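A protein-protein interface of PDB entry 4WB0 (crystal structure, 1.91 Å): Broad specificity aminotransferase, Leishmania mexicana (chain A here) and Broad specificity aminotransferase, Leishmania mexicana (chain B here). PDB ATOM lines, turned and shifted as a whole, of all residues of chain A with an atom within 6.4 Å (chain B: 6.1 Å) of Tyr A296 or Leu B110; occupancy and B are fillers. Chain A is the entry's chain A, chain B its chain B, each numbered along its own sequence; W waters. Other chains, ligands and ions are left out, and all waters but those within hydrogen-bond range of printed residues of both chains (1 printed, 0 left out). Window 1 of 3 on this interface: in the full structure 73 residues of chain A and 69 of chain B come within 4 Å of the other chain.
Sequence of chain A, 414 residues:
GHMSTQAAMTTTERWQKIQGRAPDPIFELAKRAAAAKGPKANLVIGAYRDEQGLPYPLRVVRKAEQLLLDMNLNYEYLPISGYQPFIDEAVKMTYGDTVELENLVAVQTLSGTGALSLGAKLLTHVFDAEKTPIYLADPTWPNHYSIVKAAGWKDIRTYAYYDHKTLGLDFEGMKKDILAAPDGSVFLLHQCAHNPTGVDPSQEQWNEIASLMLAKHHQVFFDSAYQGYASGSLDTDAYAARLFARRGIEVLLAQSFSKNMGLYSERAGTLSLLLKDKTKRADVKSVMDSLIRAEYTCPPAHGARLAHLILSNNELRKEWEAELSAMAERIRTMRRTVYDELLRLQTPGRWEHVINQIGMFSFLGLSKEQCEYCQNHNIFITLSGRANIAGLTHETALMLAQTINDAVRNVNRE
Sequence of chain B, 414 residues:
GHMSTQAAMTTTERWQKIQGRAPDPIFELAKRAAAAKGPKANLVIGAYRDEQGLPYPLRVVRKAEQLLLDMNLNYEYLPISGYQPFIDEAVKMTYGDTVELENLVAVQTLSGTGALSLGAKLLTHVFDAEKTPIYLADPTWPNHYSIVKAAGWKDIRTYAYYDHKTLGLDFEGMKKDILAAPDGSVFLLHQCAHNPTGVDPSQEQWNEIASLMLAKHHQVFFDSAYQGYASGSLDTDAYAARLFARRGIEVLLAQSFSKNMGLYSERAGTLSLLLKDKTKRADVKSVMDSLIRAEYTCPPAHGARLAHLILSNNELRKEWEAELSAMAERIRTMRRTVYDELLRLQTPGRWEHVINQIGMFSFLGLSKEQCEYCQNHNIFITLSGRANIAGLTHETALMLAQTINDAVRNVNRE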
ATOM      1  N   ILE A  80      -5.979  33.379  23.018  1.00  0.00           N
ATOM      2  CA  ILE A  80      -5.756  32.698  24.312  1.00  0.00           C
ATOM      3  C   ILE A  80      -7.086  32.409  24.953  1.00  0.00           C
ATOM      4  O   ILE A  80      -7.313  31.303  25.450  1.00  0.00           O
ATOM      5  CB  ILE A  80      -4.858  33.527  25.247  1.00  0.00           C
ATOM      6  CG1 ILE A  80      -3.424  33.604  24.692  1.00  0.00           C
ATOM      7  CG2 ILE A  80      -4.729  32.898  26.595  1.00  0.00           C
ATOM      8  CD1 ILE A  80      -2.640  34.685  25.315  1.00  0.00           C
ATOM      9  N   VAL A 107     -13.866  33.408  29.485  1.00  0.00           N
ATOM     10  CA  VAL A 107     -12.918  32.711  28.597  1.00  0.00           C
ATOM     11  C   VAL A 107     -13.415  31.326  28.375  1.00  0.00           C
ATOM     12  O   VAL A 107     -14.168  30.760  29.155  1.00  0.00           O
ATOM     13  CB  VAL A 107     -11.460  32.608  29.128  1.00  0.00           C
ATOM     14  CG1 VAL A 107     -10.759  34.014  29.242  1.00  0.00           C
ATOM     15  CG2 VAL A 107     -11.356  31.897  30.452  1.00  0.00           C
ATOM     16  N   GLN A 108     -12.971  30.750  27.277  1.00  0.00           N
ATOM     17  CA  GLN A 108     -13.214  29.344  27.012  1.00  0.00           C
ATOM     18  C   GLN A 108     -12.213  28.550  27.843  1.00  0.00           C
ATOM     19  O   GLN A 108     -11.051  28.975  28.022  1.00  0.00           O
ATOM     20  CB  GLN A 108     -13.046  29.069  25.529  1.00  0.00           C
ATOM     21  CG  GLN A 108     -13.265  27.577  25.096  1.00  0.00           C
ATOM     22  CD  GLN A 108     -12.938  27.337  23.567  1.00  0.00           C
ATOM     23  OE1 GLN A 108     -13.036  28.243  22.740  1.00  0.00           O
ATOM     24  NE2 GLN A 108     -12.538  26.141  23.240  1.00  0.00           N
ATOM     25  N   THR A 109     -12.627  27.392  28.317  1.00  0.00           N
ATOM     26  CA  THR A 109     -11.766  26.517  29.118  1.00  0.00           C
ATOM     27  C   THR A 109     -11.890  25.088  28.635  1.00  0.00           C
ATOM     28  O   THR A 109     -12.742  24.797  27.812  1.00  0.00           O
ATOM     29  CB  THR A 109     -12.176  26.555  30.597  1.00  0.00           C
ATOM     30  OG1 THR A 109     -13.550  26.194  30.625  1.00  0.00           O
ATOM     31  CG2 THR A 109     -12.068  27.938  31.158  1.00  0.00           C
ATOM     32  N   LEU A 110     -11.044  24.200  29.188  1.00  0.00           N
ATOM     33  CA  LEU A 110     -11.095  22.776  28.954  1.00  0.00           C
ATOM     34  C   LEU A 110     -12.201  22.161  29.782  1.00  0.00           C
ATOM     35  O   LEU A 110     -11.953  21.436  30.759  1.00  0.00           O
ATOM     36  CB  LEU A 110      -9.747  22.094  29.280  1.00  0.00           C
ATOM     37  CG  LEU A 110      -8.694  22.113  28.171  1.00  0.00           C
ATOM     38  CD1 LEU A 110      -9.210  21.344  26.974  1.00  0.00           C
ATOM     39  CD2 LEU A 110      -8.373  23.433  27.603  1.00  0.00           C
ATOM     40  N   GLY A 114     -11.345  22.188  33.611  1.00  0.00           N
ATOM     41  CA  GLY A 114     -10.491  23.291  33.217  1.00  0.00           C
ATOM     42  C   GLY A 114     -10.917  24.632  33.793  1.00  0.00           C
ATOM     43  O   GLY A 114     -10.056  25.398  34.242  1.00  0.00           O
ATOM     44  N   LEU A 118      -8.656  26.645  36.469  1.00  0.00           N
ATOM     45  CA  LEU A 118      -8.332  28.016  36.113  1.00  0.00           C
ATOM     46  C   LEU A 118      -8.908  29.020  37.118  1.00  0.00           C
ATOM     47  O   LEU A 118      -8.200  29.929  37.552  1.00  0.00           O
ATOM     48  CB  LEU A 118      -8.862  28.352  34.717  1.00  0.00           C
ATOM     49  CG  LEU A 118      -8.529  29.734  34.221  1.00  0.00           C
ATOM     50  CD1 LEU A 118      -7.024  29.952  34.155  1.00  0.00           C
ATOM     51  CD2 LEU A 118      -9.182  29.972  32.813  1.00  0.00           C
ATOM     52  N   LEU A 291      -2.256  32.815  32.818  1.00  0.00           N
ATOM     53  CA  LEU A 291      -2.397  31.479  33.397  1.00  0.00           C
ATOM     54  C   LEU A 291      -2.600  30.463  32.288  1.00  0.00           C
ATOM     55  O   LEU A 291      -2.072  29.354  32.328  1.00  0.00           O
ATOM     56  CB  LEU A 291      -3.579  31.430  34.376  1.00  0.00           C
ATOM     57  CG  LEU A 291      -3.264  32.119  35.720  1.00  0.00           C
ATOM     58  CD1 LEU A 291      -4.566  32.231  36.524  1.00  0.00           C
ATOM     59  CD2 LEU A 291      -2.255  31.336  36.508  1.00  0.00           C
ATOM     60  N   ILE A 292      -3.418  30.821  31.307  1.00  0.00           N
ATOM     61  CA  ILE A 292      -3.686  29.883  30.191  1.00  0.00           C
ATOM     62  C   ILE A 292      -2.464  29.723  29.313  1.00  0.00           C
ATOM     63  O   ILE A 292      -2.132  28.593  28.862  1.00  0.00           O
ATOM     64  CB  ILE A 292      -4.892  30.359  29.342  1.00  0.00           C
ATOM     65  CG1 ILE A 292      -6.213  30.189  30.105  1.00  0.00           C
ATOM     66  CG2 ILE A 292      -4.934  29.603  27.937  1.00  0.00           C
ATOM     67  CD1 ILE A 292      -7.362  31.100  29.508  1.00  0.00           C
ATOM     68  N   ARG A 293      -1.764  30.822  29.065  1.00  0.00           N
ATOM     69  CA  ARG A 293      -0.618  30.836  28.156  1.00  0.00           C
ATOM     70  C   ARG A 293       0.488  29.919  28.663  1.00  0.00           C
ATOM     71  O   ARG A 293       1.142  29.204  27.877  1.00  0.00           O
ATOM     72  CB  ARG A 293      -0.075  32.262  27.995  1.00  0.00           C
ATOM     73  CG  ARG A 293       1.103  32.404  27.029  1.00  0.00           C
ATOM     74  CD  ARG A 293       0.620  32.375  25.598  1.00  0.00           C
ATOM     75  NE  ARG A 293       1.705  32.778  24.708  1.00  0.00           N
ATOM     76  CZ  ARG A 293       2.184  32.061  23.695  1.00  0.00           C
ATOM     77  NH1 ARG A 293       1.687  30.851  23.372  1.00  0.00           N
ATOM     78  NH2 ARG A 293       3.183  32.573  23.003  1.00  0.00           N
ATOM     79  N   ALA A 294       0.708  29.915  29.969  1.00  0.00           N
ATOM     80  CA  ALA A 294       1.725  29.062  30.530  1.00  0.00           C
ATOM     81  C   ALA A 294       1.346  27.595  30.735  1.00  0.00           C
ATOM     82  O   ALA A 294       2.217  26.789  31.144  1.00  0.00           O
ATOM     83  CB  ALA A 294       2.201  29.643  31.857  1.00  0.00           C
ATOM     84  N   GLU A 295       0.095  27.247  30.481  1.00  0.00           N
ATOM     85  CA  GLU A 295      -0.358  25.843  30.554  1.00  0.00           C
ATOM     86  C   GLU A 295      -0.576  25.179  29.218  1.00  0.00           C
ATOM     87  O   GLU A 295      -0.133  24.075  29.061  1.00  0.00           O
ATOM     88  CB  GLU A 295      -1.666  25.717  31.311  1.00  0.00           C
ATOM     89  CG  GLU A 295      -1.560  25.885  32.798  1.00  0.00           C
ATOM     90  CD  GLU A 295      -1.021  24.625  33.528  1.00  0.00           C
ATOM     91  OE1 GLU A 295      -1.168  23.486  33.008  1.00  0.00           O
ATOM     92  OE2 GLU A 295      -0.494  24.777  34.655  1.00  0.00           O
ATOM     93  N   TYR A 296      -1.292  25.836  28.277  1.00  0.00           N
ATOM     94  CA  TYR A 296      -1.732  25.165  27.043  1.00  0.00           C
ATOM     95  C   TYR A 296      -1.908  26.137  25.871  1.00  0.00           C
ATOM     96  O   TYR A 296      -2.317  25.688  24.781  1.00  0.00           O
ATOM     97  CB  TYR A 296      -3.034  24.333  27.240  1.00  0.00           C
ATOM     98  CG  TYR A 296      -4.252  25.083  27.683  1.00  0.00           C
ATOM     99  CD1 TYR A 296      -5.083  25.666  26.762  1.00  0.00           C
ATOM    100  CD2 TYR A 296      -4.600  25.161  29.025  1.00  0.00           C
ATOM    101  CE1 TYR A 296      -6.187  26.393  27.153  1.00  0.00           C
ATOM    102  CE2 TYR A 296      -5.711  25.912  29.456  1.00  0.00           C
ATOM    103  CZ  TYR A 296      -6.514  26.508  28.508  1.00  0.00           C
ATOM    104  OH  TYR A 296      -7.638  27.243  28.843  1.00  0.00           O
ATOM    105  N   THR A 297      -1.528  27.413  26.078  1.00  0.00           N
ATOM    106  CA  THR A 297      -1.423  28.448  25.020  1.00  0.00           C
ATOM    107  C   THR A 297      -2.781  28.850  24.446  1.00  0.00           C
ATOM    108  O   THR A 297      -3.125  30.031  24.439  1.00  0.00           O
ATOM    109  CB  THR A 297      -0.496  27.992  23.864  1.00  0.00           C
ATOM    110  OG1 THR A 297       0.851  28.159  24.267  1.00  0.00           O
ATOM    111  CG2 THR A 297      -0.704  28.848  22.590  1.00  0.00           C
ATOM    112  N   CSO A 298      -3.579  27.889  24.015  1.00  0.00           N
ATOM    113  CA  CSO A 298      -4.959  28.238  23.696  1.00  0.00           C
ATOM    114  CB  CSO A 298      -5.017  29.107  22.437  1.00  0.00           C
ATOM    115  SG  CSO A 298      -4.453  28.124  21.014  1.00  0.00           S
ATOM    116  C   CSO A 298      -5.841  26.976  23.560  1.00  0.00           C
ATOM    117  O   CSO A 298      -5.333  25.880  23.412  1.00  0.00           O
ATOM    118  OD  CSO A 298      -5.917  27.600  20.133  1.00  0.00           O
ATOM    119  N   PRO A 299      -7.173  27.133  23.654  1.00  0.00           N
ATOM    120  CA  PRO A 299      -8.012  25.939  23.797  1.00  0.00           C
ATOM    121  C   PRO A 299      -8.394  25.298  22.473  1.00  0.00           C
ATOM    122  O   PRO A 299      -8.209  25.947  21.419  1.00  0.00           O
ATOM    123  CB  PRO A 299      -9.254  26.467  24.505  1.00  0.00           C
ATOM    124  CG  PRO A 299      -9.412  27.889  23.924  1.00  0.00           C
ATOM    125  CD  PRO A 299      -7.958  28.385  23.686  1.00  0.00           C
ATOM    126  N   PRO A 300      -8.868  24.032  22.507  1.00  0.00           N
ATOM    127  CA  PRO A 300      -9.240  23.320  21.284  1.00  0.00           C
ATOM    128  C   PRO A 300     -10.524  23.876  20.691  1.00  0.00           C
ATOM    129  O   PRO A 300     -11.535  24.123  21.405  1.00  0.00           O
ATOM    130  CB  PRO A 300      -9.421  21.887  21.744  1.00  0.00           C
ATOM    131  CG  PRO A 300      -9.752  22.006  23.200  1.00  0.00           C
ATOM    132  CD  PRO A 300      -9.216  23.265  23.719  1.00  0.00           C
ATOM    133  N   GLN B 108      -0.885  11.786  25.831  1.00  0.00           N
ATOM    134  CA  GLN B 108      -1.363  12.818  24.961  1.00  0.00           C
ATOM    135  C   GLN B 108      -1.362  14.128  25.764  1.00  0.00           C
ATOM    136  O   GLN B 108      -1.634  14.105  26.952  1.00  0.00           O
ATOM    137  CB  GLN B 108      -2.775  12.451  24.466  1.00  0.00           C
ATOM    138  CG  GLN B 108      -3.414  13.525  23.548  1.00  0.00           C
ATOM    139  CD  GLN B 108      -4.797  13.095  23.093  1.00  0.00           C
ATOM    140  OE1 GLN B 108      -5.102  11.898  23.055  1.00  0.00           O
ATOM    141  NE2 GLN B 108      -5.628  14.049  22.778  1.00  0.00           N
ATOM    142  N   THR B 109      -1.124  15.248  25.109  1.00  0.00           N
ATOM    143  CA  THR B 109      -1.124  16.533  25.766  1.00  0.00           C
ATOM    144  C   THR B 109      -1.801  17.571  24.886  1.00  0.00           C
ATOM    145  O   THR B 109      -2.051  17.344  23.696  1.00  0.00           O
ATOM    146  CB  THR B 109       0.305  17.004  26.073  1.00  0.00           C
ATOM    147  OG1 THR B 109       1.047  17.000  24.831  1.00  0.00           O
ATOM    148  CG2 THR B 109       0.965  16.040  27.068  1.00  0.00           C
ATOM    149  N   LEU B 110      -2.053  18.742  25.478  1.00  0.00           N
ATOM    150  CA  LEU B 110      -2.599  19.876  24.761  1.00  0.00           C
ATOM    151  C   LEU B 110      -1.478  20.503  23.968  1.00  0.00           C
ATOM    152  O   LEU B 110      -0.995  21.578  24.282  1.00  0.00           O
ATOM    153  CB  LEU B 110      -3.223  20.860  25.713  1.00  0.00           C
ATOM    154  CG  LEU B 110      -4.314  20.288  26.594  1.00  0.00           C
ATOM    155  CD1 LEU B 110      -4.761  21.349  27.622  1.00  0.00           C
ATOM    156  CD2 LEU B 110      -5.454  19.910  25.764  1.00  0.00           C
ATOM    157  N   SER B 111      -1.137  19.813  22.898  1.00  0.00           N
ATOM    158  CA  SER B 111      -0.064  20.186  21.977  1.00  0.00           C
ATOM    159  C   SER B 111       1.309  20.307  22.695  1.00  0.00           C
ATOM    160  O   SER B 111       1.506  19.711  23.769  1.00  0.00           O
ATOM    161  CB  SER B 111      -0.445  21.475  21.237  1.00  0.00           C
ATOM    162  OG  SER B 111       0.087  21.448  19.918  1.00  0.00           O
ATOM    163  N   GLY B 112       2.254  21.021  22.086  1.00  0.00           N
ATOM    164  CA  GLY B 112       3.591  21.178  22.633  1.00  0.00           C
ATOM    165  C   GLY B 112       3.560  21.926  23.956  1.00  0.00           C
ATOM    166  O   GLY B 112       4.265  21.561  24.883  1.00  0.00           O
ATOM    167  N   THR B 113       2.789  23.001  24.004  1.00  0.00           N
ATOM    168  CA  THR B 113       2.756  23.869  25.204  1.00  0.00           C
ATOM    169  C   THR B 113       2.353  23.007  26.386  1.00  0.00           C
ATOM    170  O   THR B 113       2.934  23.069  27.452  1.00  0.00           O
ATOM    171  CB  THR B 113       1.784  24.999  25.088  1.00  0.00           C
ATOM    172  OG1 THR B 113       2.125  25.833  23.993  1.00  0.00           O
ATOM    173  CG2 THR B 113       1.698  25.828  26.428  1.00  0.00           C
ATOM    174  N   GLY B 114       1.341  22.189  26.164  1.00  0.00           N
ATOM    175  CA  GLY B 114       0.802  21.360  27.212  1.00  0.00           C
ATOM    176  C   GLY B 114       1.824  20.352  27.639  1.00  0.00           C
ATOM    177  O   GLY B 114       1.944  20.036  28.829  1.00  0.00           O
ATOM    178  N   ALA B 115       2.566  19.789  26.668  1.00  0.00           N
ATOM    179  CA  ALA B 115       3.563  18.823  27.010  1.00  0.00           C
ATOM    180  C   ALA B 115       4.712  19.469  27.779  1.00  0.00           C
ATOM    181  O   ALA B 115       5.305  18.816  28.670  1.00  0.00           O
ATOM    182  CB  ALA B 115       4.111  18.123  25.767  1.00  0.00           C
ATOM    183  N   SER B 117       4.485  22.172  29.756  1.00  0.00           N
ATOM    184  CA  SER B 117       4.069  22.478  31.122  1.00  0.00           C
ATOM    185  C   SER B 117       3.999  21.191  31.950  1.00  0.00           C
ATOM    186  O   SER B 117       4.523  21.125  33.056  1.00  0.00           O
ATOM    187  CB  SER B 117       2.720  23.215  31.147  1.00  0.00           C
ATOM    188  OG  SER B 117       1.673  22.434  30.595  1.00  0.00           O
ATOM    189  N   ARG B 267      -4.936  21.365  19.070  1.00  0.00           N
ATOM    190  CA  ARG B 267      -4.092  21.090  20.233  1.00  0.00           C
ATOM    191  C   ARG B 267      -3.714  19.617  20.453  1.00  0.00           C
ATOM    192  O   ARG B 267      -4.038  19.049  21.479  1.00  0.00           O
ATOM    193  CB  ARG B 267      -4.781  21.584  21.512  1.00  0.00           C
ATOM    194  CG  ARG B 267      -5.612  22.853  21.347  1.00  0.00           C
ATOM    195  CD  ARG B 267      -4.793  24.097  20.908  1.00  0.00           C
ATOM    196  NE  ARG B 267      -3.640  24.386  21.744  1.00  0.00           N
ATOM    197  CZ  ARG B 267      -2.378  24.502  21.342  1.00  0.00           C
ATOM    198  NH1 ARG B 267      -2.041  24.370  20.055  1.00  0.00           N
ATOM    199  NH2 ARG B 267      -1.416  24.737  22.256  1.00  0.00           N
ATOM    200  N   ALA B 268      -3.015  19.029  19.511  1.00  0.00           N
ATOM    201  CA  ALA B 268      -2.591  17.645  19.602  1.00  0.00           C
ATOM    202  C   ALA B 268      -1.069  17.537  19.802  1.00  0.00           C
ATOM    203  O   ALA B 268      -0.292  18.106  19.006  1.00  0.00           O
ATOM    204  CB  ALA B 268      -3.031  16.890  18.323  1.00  0.00           C
ATOM    205  N   GLY B 269      -0.650  16.872  20.883  1.00  0.00           N
ATOM    206  CA  GLY B 269       0.777  16.689  21.163  1.00  0.00           C
ATOM    207  C   GLY B 269       0.957  15.518  22.068  1.00  0.00           C
ATOM    208  O   GLY B 269      -0.014  14.868  22.411  1.00  0.00           O
ATOM    209  N   TYR B 296      -7.328  19.243  33.777  1.00  0.00           N
ATOM    210  CA  TYR B 296      -8.383  19.223  32.739  1.00  0.00           C
ATOM    211  C   TYR B 296      -9.064  17.874  32.539  1.00  0.00           C
ATOM    212  O   TYR B 296      -9.816  17.696  31.595  1.00  0.00           O
ATOM    213  CB  TYR B 296      -7.840  19.751  31.376  1.00  0.00           C
ATOM    214  CG  TYR B 296      -6.666  18.989  30.808  1.00  0.00           C
ATOM    215  CD1 TYR B 296      -6.849  17.843  30.057  1.00  0.00           C
ATOM    216  CD2 TYR B 296      -5.345  19.380  31.095  1.00  0.00           C
ATOM    217  CE1 TYR B 296      -5.765  17.125  29.559  1.00  0.00           C
ATOM    218  CE2 TYR B 296      -4.243  18.645  30.580  1.00  0.00           C
ATOM    219  CZ  TYR B 296      -4.472  17.534  29.808  1.00  0.00           C
ATOM    220  OH  TYR B 296      -3.416  16.752  29.294  1.00  0.00           O
ATOM    221  N   PRO B 299      -7.886  14.708  27.689  1.00  0.00           N
ATOM    222  CA  PRO B 299      -7.607  15.646  26.595  1.00  0.00           C
ATOM    223  C   PRO B 299      -8.675  15.621  25.507  1.00  0.00           C
ATOM    224  O   PRO B 299      -9.444  14.684  25.431  1.00  0.00           O
ATOM    225  CB  PRO B 299      -6.267  15.148  26.035  1.00  0.00           C
ATOM    226  CG  PRO B 299      -6.327  13.662  26.315  1.00  0.00           C
ATOM    227  CD  PRO B 299      -7.079  13.480  27.597  1.00  0.00           C
ATOM    228  N   PRO B 300      -8.711  16.635  24.649  1.00  0.00           N
ATOM    229  CA  PRO B 300      -9.714  16.592  23.594  1.00  0.00           C
ATOM    230  C   PRO B 300      -9.381  15.570  22.524  1.00  0.00           C
ATOM    231  O   PRO B 300      -8.186  15.407  22.214  1.00  0.00           O
ATOM    232  CB  PRO B 300      -9.665  17.997  22.978  1.00  0.00           C
ATOM    233  CG  PRO B 300      -8.321  18.528  23.338  1.00  0.00           C
ATOM    234  CD  PRO B 300      -7.934  17.879  24.643  1.00  0.00           C
HETATM  235  O   HOH W   1       0.180  21.021  32.799  1.00  0.00           O
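The side-chain hydroxyl of Ser B117 sits at hydrogen-bond distance from the backbone carbonyl oxygen of Glu A295, at 2.9 Å. O of Tyr A296 lies within hydrogen-bond range of NH2 of Arg B267 (2.8 Å). OG1 of Thr A297 lies within hydrogen-bond range of OG1 of Thr B113 (2.7 Å). O of CSO A298 lies within hydrogen-bond range of the guanidinium group (NE) of Arg B267 (2.8 Å).
Water W1 lies within hydrogen-bond range of OE1 of Glu A295 (2.8 Å) and OG of Ser B117 (3.0 Å).
Among the printed residues, merely in contact across the chains: Leu A110 with Tyr B296, Arg A293 with Thr B113, Ala A294 with Ser B117, Glu A295 with Thr B113, Glu A295 with Gly B114, Tyr A296 with Leu B110, Tyr A296 with Thr B113, Thr A297 with Arg B267, Pro A299 with Arg B267, Pro A300 with Arg B267 and Pro A300 with Pro B300.
The side-chain amide nitrogen (NE2) of Gln A108 sits at hydrogen-bond distance from the backbone carbonyl oxygen (O) of Pro A300 (2.9 Å). The backbone carbonyl oxygen of Ile A292 lies within hydrogen-bond range of the backbone NH of Thr A297. The guanidinium group (NH1) of Arg A293 lies within hydrogen-bond range of the side-chain hydroxyl (OG1) of Thr A297 (3.0 Å). The side-chain amide nitrogen (NE2) of Gln B108 lies within hydrogen-bond range of the backbone carbonyl oxygen (O) of Pro B300, 3.0 Å away. O of Thr B113 is in hydrogen-bond range of OG of Ser B117, at 3.4 Å. The side-chain hydroxyl (OG) of Ser B117 lies within hydrogen-bond range of the backbone carbonyl oxygen (O) of Gly B114.
Along chain A the printed residues that touch a printed residue of chain B span positions 110 to 300. Of the 15 printed residues of chain B, 7 touch a printed residue of chain A. Hydrophobic or aromatic side chains of chain B that line the printed part of chain A: Leu B110, Tyr B296 and Pro B300. Among the printed residues, no Asp or Glu carboxylate lies within 4 Å of a Lys or Arg side-chain nitrogen of the other chain.
Of the printed residues of chain B, Pro A299 touches Arg B267. Leu B110 touches just one residue of chain A: Tyr A296 (3.5 Å). Ser B111 touches none of the printed residues of chain A. Printed residues of chain A within 4 Å of Thr B113: Arg A293, Glu A295, Tyr A296 and Thr A297. Printed residues of chain A within 4 Å of Ser B117: Ala A294 and Glu A295. Printed residues of chain A within 4 Å of Tyr B296: Leu A110. The nearest residue of chain A that does not touch Leu B110 is Leu A110 (4.04 Å). The nearest printed residue of chain A that does not touch Pro B300 is Leu A110 (4.4 Å).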
